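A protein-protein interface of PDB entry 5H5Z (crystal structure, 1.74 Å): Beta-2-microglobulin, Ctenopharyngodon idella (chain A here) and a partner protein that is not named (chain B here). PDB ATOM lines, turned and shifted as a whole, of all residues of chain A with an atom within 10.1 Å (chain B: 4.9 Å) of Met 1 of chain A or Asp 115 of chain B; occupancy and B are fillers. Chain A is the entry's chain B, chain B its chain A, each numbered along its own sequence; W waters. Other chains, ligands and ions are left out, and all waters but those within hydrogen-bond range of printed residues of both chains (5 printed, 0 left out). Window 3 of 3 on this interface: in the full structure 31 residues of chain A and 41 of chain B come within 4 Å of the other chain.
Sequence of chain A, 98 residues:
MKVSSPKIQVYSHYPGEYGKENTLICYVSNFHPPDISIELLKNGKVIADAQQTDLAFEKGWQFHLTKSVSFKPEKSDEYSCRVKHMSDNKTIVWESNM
ND1 of His 90 of chain B is in hydrogen-bond range of OD2 of Asp 115 of chain B (2.8 Å). The backbone carbonyl oxygen (O) of Thr 91 of chain B is in hydrogen-bond range of the backbone NH (N) of Asp 115 of chain B. The backbone NH (N) of Ser 4 of chain A is in hydrogen-bond range of the backbone carbonyl oxygen (O) of His 32 of chain A (2.8 Å).
Water W2 bridges O of Asp 115 of chain B (2.7 Å) and N of Lys 2 of chain A (2.8 Å). Water W3 bridges O of Gly 116 of chain B (2.8 Å) and O of Gly 60 of chain A (3.0 Å). Water W5 bridges the side-chain carboxylate (OD1) of Asp 115 of chain B (2.8 Å) and a ring nitrogen (NE2) of His 32 of chain A (2.8 Å). Water W1 bridges the backbone NH of Met 1 of chain A (2.8 Å) and the side-chain carboxylate of Glu 117 of chain B (3.4 Å). Water W4 lies within hydrogen-bond range of OD2 of Asp 115 of chain B, N of Met 1 of chain A and NE2 of Gln 85 of chain B.
The backbone carbonyl oxygen (O) of Asp 115 of chain B lies within hydrogen-bond range of a ring nitrogen (NE2) of His 32 of chain A, 3.1 Å away.
Met 1 of chain A touches one residue of chain B. Of chain A, only Met 1 and His 32 come within 4 Å of Asp 115 of chain B. No residue of chain A comes within 4 Å of His 90 of chain B. Thr 91 of chain B touches two residues of chain A. No residue of chain A comes within 4 Å of Tyr 114 of chain B. Of the printed residues of chain B, His 32 of chain A touches Thr 91, Asp 115 and Gly 116. Printed residues of chain B within 4 Å of Gly 60 of chain A: Gly 116 (3.98 Å). Of the printed residues of chain B, Pro 34 of chain A touches Thr 91. Of the printed residues of chain B, Trp 61 of chain A touches Ala 113 (3.3 Å) and Gly 116 (3.7 Å). The nearest residue of chain B that does not touch Met 1 of chain A is Gln 85 of chain B (4.4 Å). The nearest residue of chain A that does not touch Asp 115 of chain B is Lys 2 of chain A (5.1 Å). The nearest printed residue of chain B that does not touch Trp 61 of chain A is Glu 117 of chain B (4.4 Å).
Among the printed residues, pairs that only touch across the chains: Met 1 of chain A with Asp 115 of chain B, His 32 of chain A with Thr 91 of chain B, His 32 of chain A with Gly 116 of chain B, Pro 34 of chain A with Thr 91 of chain B, Gly 60 of chain A with Gly 116 of chain B, Trp 61 of chain A with Ala 113 of chain B and Trp 61 of chain A with Gly 116 of chain B.
Of the 9 printed residues of chain B, 4 touch a printed residue of chain A. Hydrophobic or aromatic side chains of chain B that line the printed part of chain A: Ala 113. Of the 17 printed residues of chain A, 5 touch a printed residue of chain B. Hydrophobic or aromatic side chains of chain A that line the printed part of chain B: Met 1, His 32, Pro 34 and Trp 61. Among the printed residues, no Asp or Glu carboxylate lies within 4 Å of a Lys or Arg side-chain nitrogen of the other chain.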
ATOM      1  N   MET A   1      19.122   9.543  16.754  1.00  0.00           N
ATOM      2  CA  MET A   1      18.711   8.942  15.455  1.00  0.00           C
ATOM      3  C   MET A   1      17.408   8.157  15.609  1.00  0.00           C
ATOM      4  O   MET A   1      17.262   7.377  16.546  1.00  0.00           O
ATOM      5  CB  MET A   1      19.829   8.041  14.916  1.00  0.00           C
ATOM      6  CG  MET A   1      19.567   7.442  13.543  1.00  0.00           C
ATOM      7  SD  MET A   1      18.612   5.913  13.605  1.00  0.00           S
ATOM      8  CE  MET A   1      18.438   5.571  11.856  1.00  0.00           C
ATOM      9  N   LYS A   2      16.477   8.368  14.682  1.00  0.00           N
ATOM     10  CA  LYS A   2      15.221   7.622  14.648  1.00  0.00           C
ATOM     11  C   LYS A   2      14.918   7.202  13.210  1.00  0.00           C
ATOM     12  O   LYS A   2      15.164   7.963  12.268  1.00  0.00           O
ATOM     13  CB  LYS A   2      14.080   8.475  15.213  1.00  0.00           C
ATOM     14  CG  LYS A   2      12.765   7.734  15.404  1.00  0.00           C
ATOM     15  CD  LYS A   2      11.661   8.640  15.931  1.00  0.00           C
ATOM     16  CE  LYS A   2      11.897   9.027  17.384  1.00  0.00           C
ATOM     17  NZ  LYS A   2      10.636   9.439  18.060  1.00  0.00           N
ATOM     18  N   VAL A   3      14.401   5.987  13.046  1.00  0.00           N
ATOM     19  CA  VAL A   3      13.980   5.501  11.736  1.00  0.00           C
ATOM     20  C   VAL A   3      12.600   6.063  11.396  1.00  0.00           C
ATOM     21  O   VAL A   3      11.717   6.117  12.253  1.00  0.00           O
ATOM     22  CB  VAL A   3      13.942   3.955  11.674  1.00  0.00           C
ATOM     23  CG1 VAL A   3      13.460   3.473  10.311  1.00  0.00           C
ATOM     24  CG2 VAL A   3      15.313   3.370  11.974  1.00  0.00           C
ATOM     25  N   SER A   4      12.438   6.503  10.150  1.00  0.00           N
ATOM     26  CA  SER A   4      11.129   6.817   9.590  1.00  0.00           C
ATOM     27  C   SER A   4      10.857   5.803   8.495  1.00  0.00           C
ATOM     28  O   SER A   4      11.544   5.793   7.473  1.00  0.00           O
ATOM     29  CB  SER A   4      11.095   8.237   9.017  1.00  0.00           C
ATOM     30  OG  SER A   4      11.113   9.208  10.048  1.00  0.00           O
ATOM     31  N   SER A   5       9.874   4.936   8.720  1.00  0.00           N
ATOM     32  CA  SER A   5       9.534   3.889   7.761  1.00  0.00           C
ATOM     33  C   SER A   5       8.742   4.458   6.589  1.00  0.00           C
ATOM     34  O   SER A   5       7.901   5.331   6.782  1.00  0.00           O
ATOM     35  CB  SER A   5       8.761   2.762   8.448  1.00  0.00           C
ATOM     36  OG  SER A   5       9.598   2.105   9.383  1.00  0.00           O
ATOM     37  N   PHE A  31      10.670   8.701   4.327  1.00  0.00           N
ATOM     38  CA  PHE A  31      11.567   7.724   4.949  1.00  0.00           C
ATOM     39  C   PHE A  31      12.962   8.246   5.287  1.00  0.00           C
ATOM     40  O   PHE A  31      13.488   9.124   4.615  1.00  0.00           O
ATOM     41  CB  PHE A  31      11.639   6.422   4.132  1.00  0.00           C
ATOM     42  CG  PHE A  31      12.359   6.551   2.816  1.00  0.00           C
ATOM     43  CD1 PHE A  31      13.734   6.331   2.731  1.00  0.00           C
ATOM     44  CD2 PHE A  31      11.659   6.854   1.651  1.00  0.00           C
ATOM     45  CE1 PHE A  31      14.398   6.436   1.516  1.00  0.00           C
ATOM     46  CE2 PHE A  31      12.316   6.960   0.435  1.00  0.00           C
ATOM     47  CZ  PHE A  31      13.689   6.754   0.367  1.00  0.00           C
ATOM     48  N   HIS A  32      13.531   7.693   6.358  1.00  0.00           N
ATOM     49  CA  HIS A  32      14.895   7.992   6.808  1.00  0.00           C
ATOM     50  C   HIS A  32      15.363   6.794   7.633  1.00  0.00           C
ATOM     51  O   HIS A  32      14.581   6.267   8.421  1.00  0.00           O
ATOM     52  CB  HIS A  32      14.918   9.252   7.676  1.00  0.00           C
ATOM     53  CG  HIS A  32      16.234   9.503   8.350  1.00  0.00           C
ATOM     54  ND1 HIS A  32      17.281  10.141   7.721  1.00  0.00           N
ATOM     55  CD2 HIS A  32      16.675   9.193   9.594  1.00  0.00           C
ATOM     56  CE1 HIS A  32      18.308  10.218   8.547  1.00  0.00           C
ATOM     57  NE2 HIS A  32      17.968   9.648   9.690  1.00  0.00           N
ATOM     58  N   PRO A  33      16.635   6.356   7.471  1.00  0.00           N
ATOM     59  CA  PRO A  33      17.696   6.881   6.593  1.00  0.00           C
ATOM     60  C   PRO A  33      17.487   6.534   5.103  1.00  0.00           C
ATOM     61  O   PRO A  33      16.561   5.787   4.777  1.00  0.00           O
ATOM     62  CB  PRO A  33      18.963   6.229   7.155  1.00  0.00           C
ATOM     63  CG  PRO A  33      18.493   4.948   7.745  1.00  0.00           C
ATOM     64  CD  PRO A  33      17.122   5.228   8.294  1.00  0.00           C
ATOM     65  N   PRO A  34      18.341   7.077   4.212  1.00  0.00           N
ATOM     66  CA  PRO A  34      18.094   7.017   2.761  1.00  0.00           C
ATOM     67  C   PRO A  34      18.284   5.662   2.077  1.00  0.00           C
ATOM     68  O   PRO A  34      17.650   5.420   1.046  1.00  0.00           O
ATOM     69  CB  PRO A  34      19.083   8.037   2.190  1.00  0.00           C
ATOM     70  CG  PRO A  34      20.179   8.116   3.197  1.00  0.00           C
ATOM     71  CD  PRO A  34      19.521   7.905   4.530  1.00  0.00           C
ATOM     72  N   ASP A  35      19.144   4.801   2.620  1.00  0.00           N
ATOM     73  CA  ASP A  35      19.402   3.497   2.011  1.00  0.00           C
ATOM     74  C   ASP A  35      18.130   2.665   1.955  1.00  0.00           C
ATOM     75  O   ASP A  35      17.474   2.445   2.977  1.00  0.00           O
ATOM     76  CB  ASP A  35      20.493   2.738   2.765  1.00  0.00           C
ATOM     77  CG  ASP A  35      21.377   1.928   1.844  1.00  0.00           C
ATOM     78  OD1 ASP A  35      20.882   0.950   1.243  1.00  0.00           O
ATOM     79  OD2 ASP A  35      22.567   2.287   1.709  1.00  0.00           O
ATOM     80  N   GLY A  60      11.408  19.102   5.940  1.00  0.00           N
ATOM     81  CA  GLY A  60      11.228  18.093   6.977  1.00  0.00           C
ATOM     82  C   GLY A  60      12.273  16.993   6.883  1.00  0.00           C
ATOM     83  O   GLY A  60      12.392  16.166   7.794  1.00  0.00           O
ATOM     84  N   TRP A  61      13.001  16.968   5.762  1.00  0.00           N
ATOM     85  CA  TRP A  61      14.213  16.149   5.575  1.00  0.00           C
ATOM     86  C   TRP A  61      14.000  14.697   5.139  1.00  0.00           C
ATOM     87  O   TRP A  61      14.964  14.004   4.813  1.00  0.00           O
ATOM     88  CB  TRP A  61      15.105  16.176   6.826  1.00  0.00           C
ATOM     89  CG  TRP A  61      15.433  17.547   7.307  1.00  0.00           C
ATOM     90  CD1 TRP A  61      14.941  18.174   8.415  1.00  0.00           C
ATOM     91  CD2 TRP A  61      16.320  18.471   6.681  1.00  0.00           C
ATOM     92  NE1 TRP A  61      15.485  19.435   8.527  1.00  0.00           N
ATOM     93  CE2 TRP A  61      16.328  19.646   7.468  1.00  0.00           C
ATOM     94  CE3 TRP A  61      17.117  18.418   5.530  1.00  0.00           C
ATOM     95  CZ2 TRP A  61      17.111  20.756   7.148  1.00  0.00           C
ATOM     96  CZ3 TRP A  61      17.891  19.525   5.210  1.00  0.00           C
ATOM     97  CH2 TRP A  61      17.880  20.677   6.017  1.00  0.00           C
ATOM     98  N   GLN A  62      12.755  14.230   5.144  1.00  0.00           N
ATOM     99  CA  GLN A  62      12.475  12.839   4.794  1.00  0.00           C
ATOM    100  C   GLN A  62      12.612  12.625   3.286  1.00  0.00           C
ATOM    101  O   GLN A  62      12.269  13.502   2.487  1.00  0.00           O
ATOM    102  CB  GLN A  62      11.089  12.420   5.297  1.00  0.00           C
ATOM    103  CG  GLN A  62      10.927  12.563   6.808  1.00  0.00           C
ATOM    104  CD  GLN A  62       9.560  12.139   7.322  1.00  0.00           C
ATOM    105  OE1 GLN A  62       9.415  11.775   8.489  1.00  0.00           O
ATOM    106  NE2 GLN A  62       8.550  12.197   6.462  1.00  0.00           N
ATOM    107  N   PHE A  63      13.125  11.455   2.918  1.00  0.00           N
ATOM    108  CA  PHE A  63      13.462  11.135   1.532  1.00  0.00           C
ATOM    109  C   PHE A  63      12.264  10.602   0.749  1.00  0.00           C
ATOM    110  O   PHE A  63      11.323  10.056   1.324  1.00  0.00           O
ATOM    111  CB  PHE A  63      14.591  10.100   1.503  1.00  0.00           C
ATOM    112  CG  PHE A  63      15.879  10.591   2.089  1.00  0.00           C
ATOM    113  CD1 PHE A  63      16.751  11.348   1.319  1.00  0.00           C
ATOM    114  CD2 PHE A  63      16.229  10.296   3.408  1.00  0.00           C
ATOM    115  CE1 PHE A  63      17.952  11.806   1.850  1.00  0.00           C
ATOM    116  CE2 PHE A  63      17.425  10.756   3.947  1.00  0.00           C
ATOM    117  CZ  PHE A  63      18.288  11.511   3.164  1.00  0.00           C
ATOM    118  N   HIS A  85      13.569  -1.509   3.661  1.00  0.00           N
ATOM    119  CA  HIS A  85      14.174  -0.395   4.390  1.00  0.00           C
ATOM    120  C   HIS A  85      14.619  -0.897   5.755  1.00  0.00           C
ATOM    121  O   HIS A  85      13.842  -1.545   6.462  1.00  0.00           O
ATOM    122  CB  HIS A  85      13.162   0.741   4.543  1.00  0.00           C
ATOM    123  CG  HIS A  85      13.726   1.990   5.143  1.00  0.00           C
ATOM    124  ND1 HIS A  85      13.251   2.530   6.318  1.00  0.00           N
ATOM    125  CD2 HIS A  85      14.713   2.818   4.722  1.00  0.00           C
ATOM    126  CE1 HIS A  85      13.923   3.632   6.600  1.00  0.00           C
ATOM    127  NE2 HIS A  85      14.816   3.828   5.646  1.00  0.00           N
ATOM    128  N   MET A  86      15.864  -0.591   6.123  1.00  0.00           N
ATOM    129  CA  MET A  86      16.501  -1.181   7.303  1.00  0.00           C
ATOM    130  C   MET A  86      16.385  -2.705   7.201  1.00  0.00           C
ATOM    131  O   MET A  86      16.901  -3.295   6.250  1.00  0.00           O
ATOM    132  CB  MET A  86      15.880  -0.646   8.604  1.00  0.00           C
ATOM    133  CG  MET A  86      15.857   0.870   8.722  1.00  0.00           C
ATOM    134  SD  MET A  86      17.510   1.587   8.792  1.00  0.00           S
ATOM    135  CE  MET A  86      18.041   1.114  10.439  1.00  0.00           C
ATOM    136  N   SER A  87      15.686  -3.328   8.149  1.00  0.00           N
ATOM    137  CA  SER A  87      15.454  -4.774   8.114  1.00  0.00           C
ATOM    138  C   SER A  87      13.994  -5.136   7.809  1.00  0.00           C
ATOM    139  O   SER A  87      13.590  -6.296   7.935  1.00  0.00           O
ATOM    140  CB  SER A  87      15.910  -5.419   9.426  1.00  0.00           C
ATOM    141  OG  SER A  87      17.290  -5.188   9.636  1.00  0.00           O
ATOM    142  N   GLN B  85      28.633   9.323  18.760  1.00  0.00           N
ATOM    143  CA  GLN B  85      28.265   8.219  17.880  1.00  0.00           C
ATOM    144  C   GLN B  85      29.430   7.878  16.949  1.00  0.00           C
ATOM    145  O   GLN B  85      29.612   8.508  15.906  1.00  0.00           O
ATOM    146  CB  GLN B  85      27.007   8.576  17.075  1.00  0.00           C
ATOM    147  CG  GLN B  85      25.773   8.878  17.921  1.00  0.00           C
ATOM    148  CD  GLN B  85      24.687   9.617  17.150  1.00  0.00           C
ATOM    149  OE1 GLN B  85      24.966  10.310  16.173  1.00  0.00           O
ATOM    150  NE2 GLN B  85      23.443   9.477  17.594  1.00  0.00           N
ATOM    151  N   VAL B  89      25.460   3.952  10.672  1.00  0.00           N
ATOM    152  CA  VAL B  89      25.206   4.876   9.568  1.00  0.00           C
ATOM    153  C   VAL B  89      24.598   6.190  10.067  1.00  0.00           C
ATOM    154  O   VAL B  89      23.653   6.194  10.855  1.00  0.00           O
ATOM    155  CB  VAL B  89      24.329   4.224   8.461  1.00  0.00           C
ATOM    156  CG1 VAL B  89      23.027   3.670   9.029  1.00  0.00           C
ATOM    157  CG2 VAL B  89      24.056   5.201   7.323  1.00  0.00           C
ATOM    158  N   HIS B  90      25.159   7.306   9.616  1.00  0.00           N
ATOM    159  CA  HIS B  90      24.601   8.614   9.930  1.00  0.00           C
ATOM    160  C   HIS B  90      24.515   9.473   8.675  1.00  0.00           C
ATOM    161  O   HIS B  90      25.197   9.203   7.683  1.00  0.00           O
ATOM    162  CB  HIS B  90      25.397   9.293  11.047  1.00  0.00           C
ATOM    163  CG  HIS B  90      25.374   8.536  12.339  1.00  0.00           C
ATOM    164  ND1 HIS B  90      24.307   8.587  13.212  1.00  0.00           N
ATOM    165  CD2 HIS B  90      26.272   7.687  12.892  1.00  0.00           C
ATOM    166  CE1 HIS B  90      24.556   7.811  14.253  1.00  0.00           C
ATOM    167  NE2 HIS B  90      25.742   7.253  14.084  1.00  0.00           N
ATOM    168  N   THR B  91      23.654  10.486   8.719  1.00  0.00           N
ATOM    169  CA  THR B  91      23.387  11.322   7.550  1.00  0.00           C
ATOM    170  C   THR B  91      23.549  12.801   7.870  1.00  0.00           C
ATOM    171  O   THR B  91      23.279  13.245   8.993  1.00  0.00           O
ATOM    172  CB  THR B  91      21.963  11.113   6.988  1.00  0.00           C
ATOM    173  OG1 THR B  91      21.009  11.735   7.855  1.00  0.00           O
ATOM    174  CG2 THR B  91      21.624   9.635   6.849  1.00  0.00           C
ATOM    175  N   ALA B 113      20.626  19.518   8.366  1.00  0.00           N
ATOM    176  CA  ALA B 113      20.093  18.528   9.312  1.00  0.00           C
ATOM    177  C   ALA B 113      21.074  17.397   9.524  1.00  0.00           C
ATOM    178  O   ALA B 113      21.787  16.996   8.596  1.00  0.00           O
ATOM    179  CB  ALA B 113      18.763  17.962   8.827  1.00  0.00           C
ATOM    180  N   TYR B 114      21.098  16.890  10.753  1.00  0.00           N
ATOM    181  CA  TYR B 114      21.858  15.702  11.090  1.00  0.00           C
ATOM    182  C   TYR B 114      20.889  14.588  11.459  1.00  0.00           C
ATOM    183  O   TYR B 114      19.972  14.794  12.262  1.00  0.00           O
ATOM    184  CB  TYR B 114      22.816  15.982  12.248  1.00  0.00           C
ATOM    185  CG  TYR B 114      23.556  14.752  12.721  1.00  0.00           C
ATOM    186  CD1 TYR B 114      24.489  14.122  11.898  1.00  0.00           C
ATOM    187  CD2 TYR B 114      23.318  14.209  13.987  1.00  0.00           C
ATOM    188  CE1 TYR B 114      25.173  12.996  12.317  1.00  0.00           C
ATOM    189  CE2 TYR B 114      23.998  13.082  14.417  1.00  0.00           C
ATOM    190  CZ  TYR B 114      24.923  12.479  13.580  1.00  0.00           C
ATOM    191  OH  TYR B 114      25.598  11.360  14.002  1.00  0.00           O
ATOM    192  N   ASP B 115      21.103  13.412  10.870  1.00  0.00           N
ATOM    193  CA  ASP B 115      20.176  12.272  10.993  1.00  0.00           C
ATOM    194  C   ASP B 115      18.713  12.675  10.783  1.00  0.00           C
ATOM    195  O   ASP B 115      17.817  12.212  11.491  1.00  0.00           O
ATOM    196  CB  ASP B 115      20.384  11.517  12.319  1.00  0.00           C
ATOM    197  CG  ASP B 115      21.660  10.693  12.324  1.00  0.00           C
ATOM    198  OD1 ASP B 115      22.176  10.367  11.237  1.00  0.00           O
ATOM    199  OD2 ASP B 115      22.154  10.359  13.420  1.00  0.00           O
ATOM    200  N   GLY B 116      18.486  13.549   9.804  1.00  0.00           N
ATOM    201  CA  GLY B 116      17.136  13.977   9.436  1.00  0.00           C
ATOM    202  C   GLY B 116      16.429  14.892  10.423  1.00  0.00           C
ATOM    203  O   GLY B 116      15.210  15.036  10.370  1.00  0.00           O
ATOM    204  N   GLU B 117      17.190  15.504  11.327  1.00  0.00           N
ATOM    205  CA  GLU B 117      16.646  16.476  12.276  1.00  0.00           C
ATOM    206  C   GLU B 117      17.370  17.819  12.161  1.00  0.00           C
ATOM    207  O   GLU B 117      18.589  17.848  11.988  1.00  0.00           O
ATOM    208  CB  GLU B 117      16.767  15.948  13.705  1.00  0.00           C
ATOM    209  CG  GLU B 117      15.816  14.805  14.027  1.00  0.00           C
ATOM    210  CD  GLU B 117      15.866  14.410  15.489  1.00  0.00           C
ATOM    211  OE1 GLU B 117      16.975  14.146  16.004  1.00  0.00           O
ATOM    212  OE2 GLU B 117      14.796  14.362  16.124  1.00  0.00           O
HETATM  213  O   HOH W   1      16.897  11.054  17.493  1.00  0.00           O
HETATM  214  O   HOH W   2      16.734  10.850  13.512  1.00  0.00           O
HETATM  215  O   HOH W   3      13.519  13.526   8.790  1.00  0.00           O
HETATM  216  O   HOH W   4      21.395  11.229  15.961  1.00  0.00           O
HETATM  217  O   HOH W   5      20.473   8.479  10.108  1.00  0.00           O
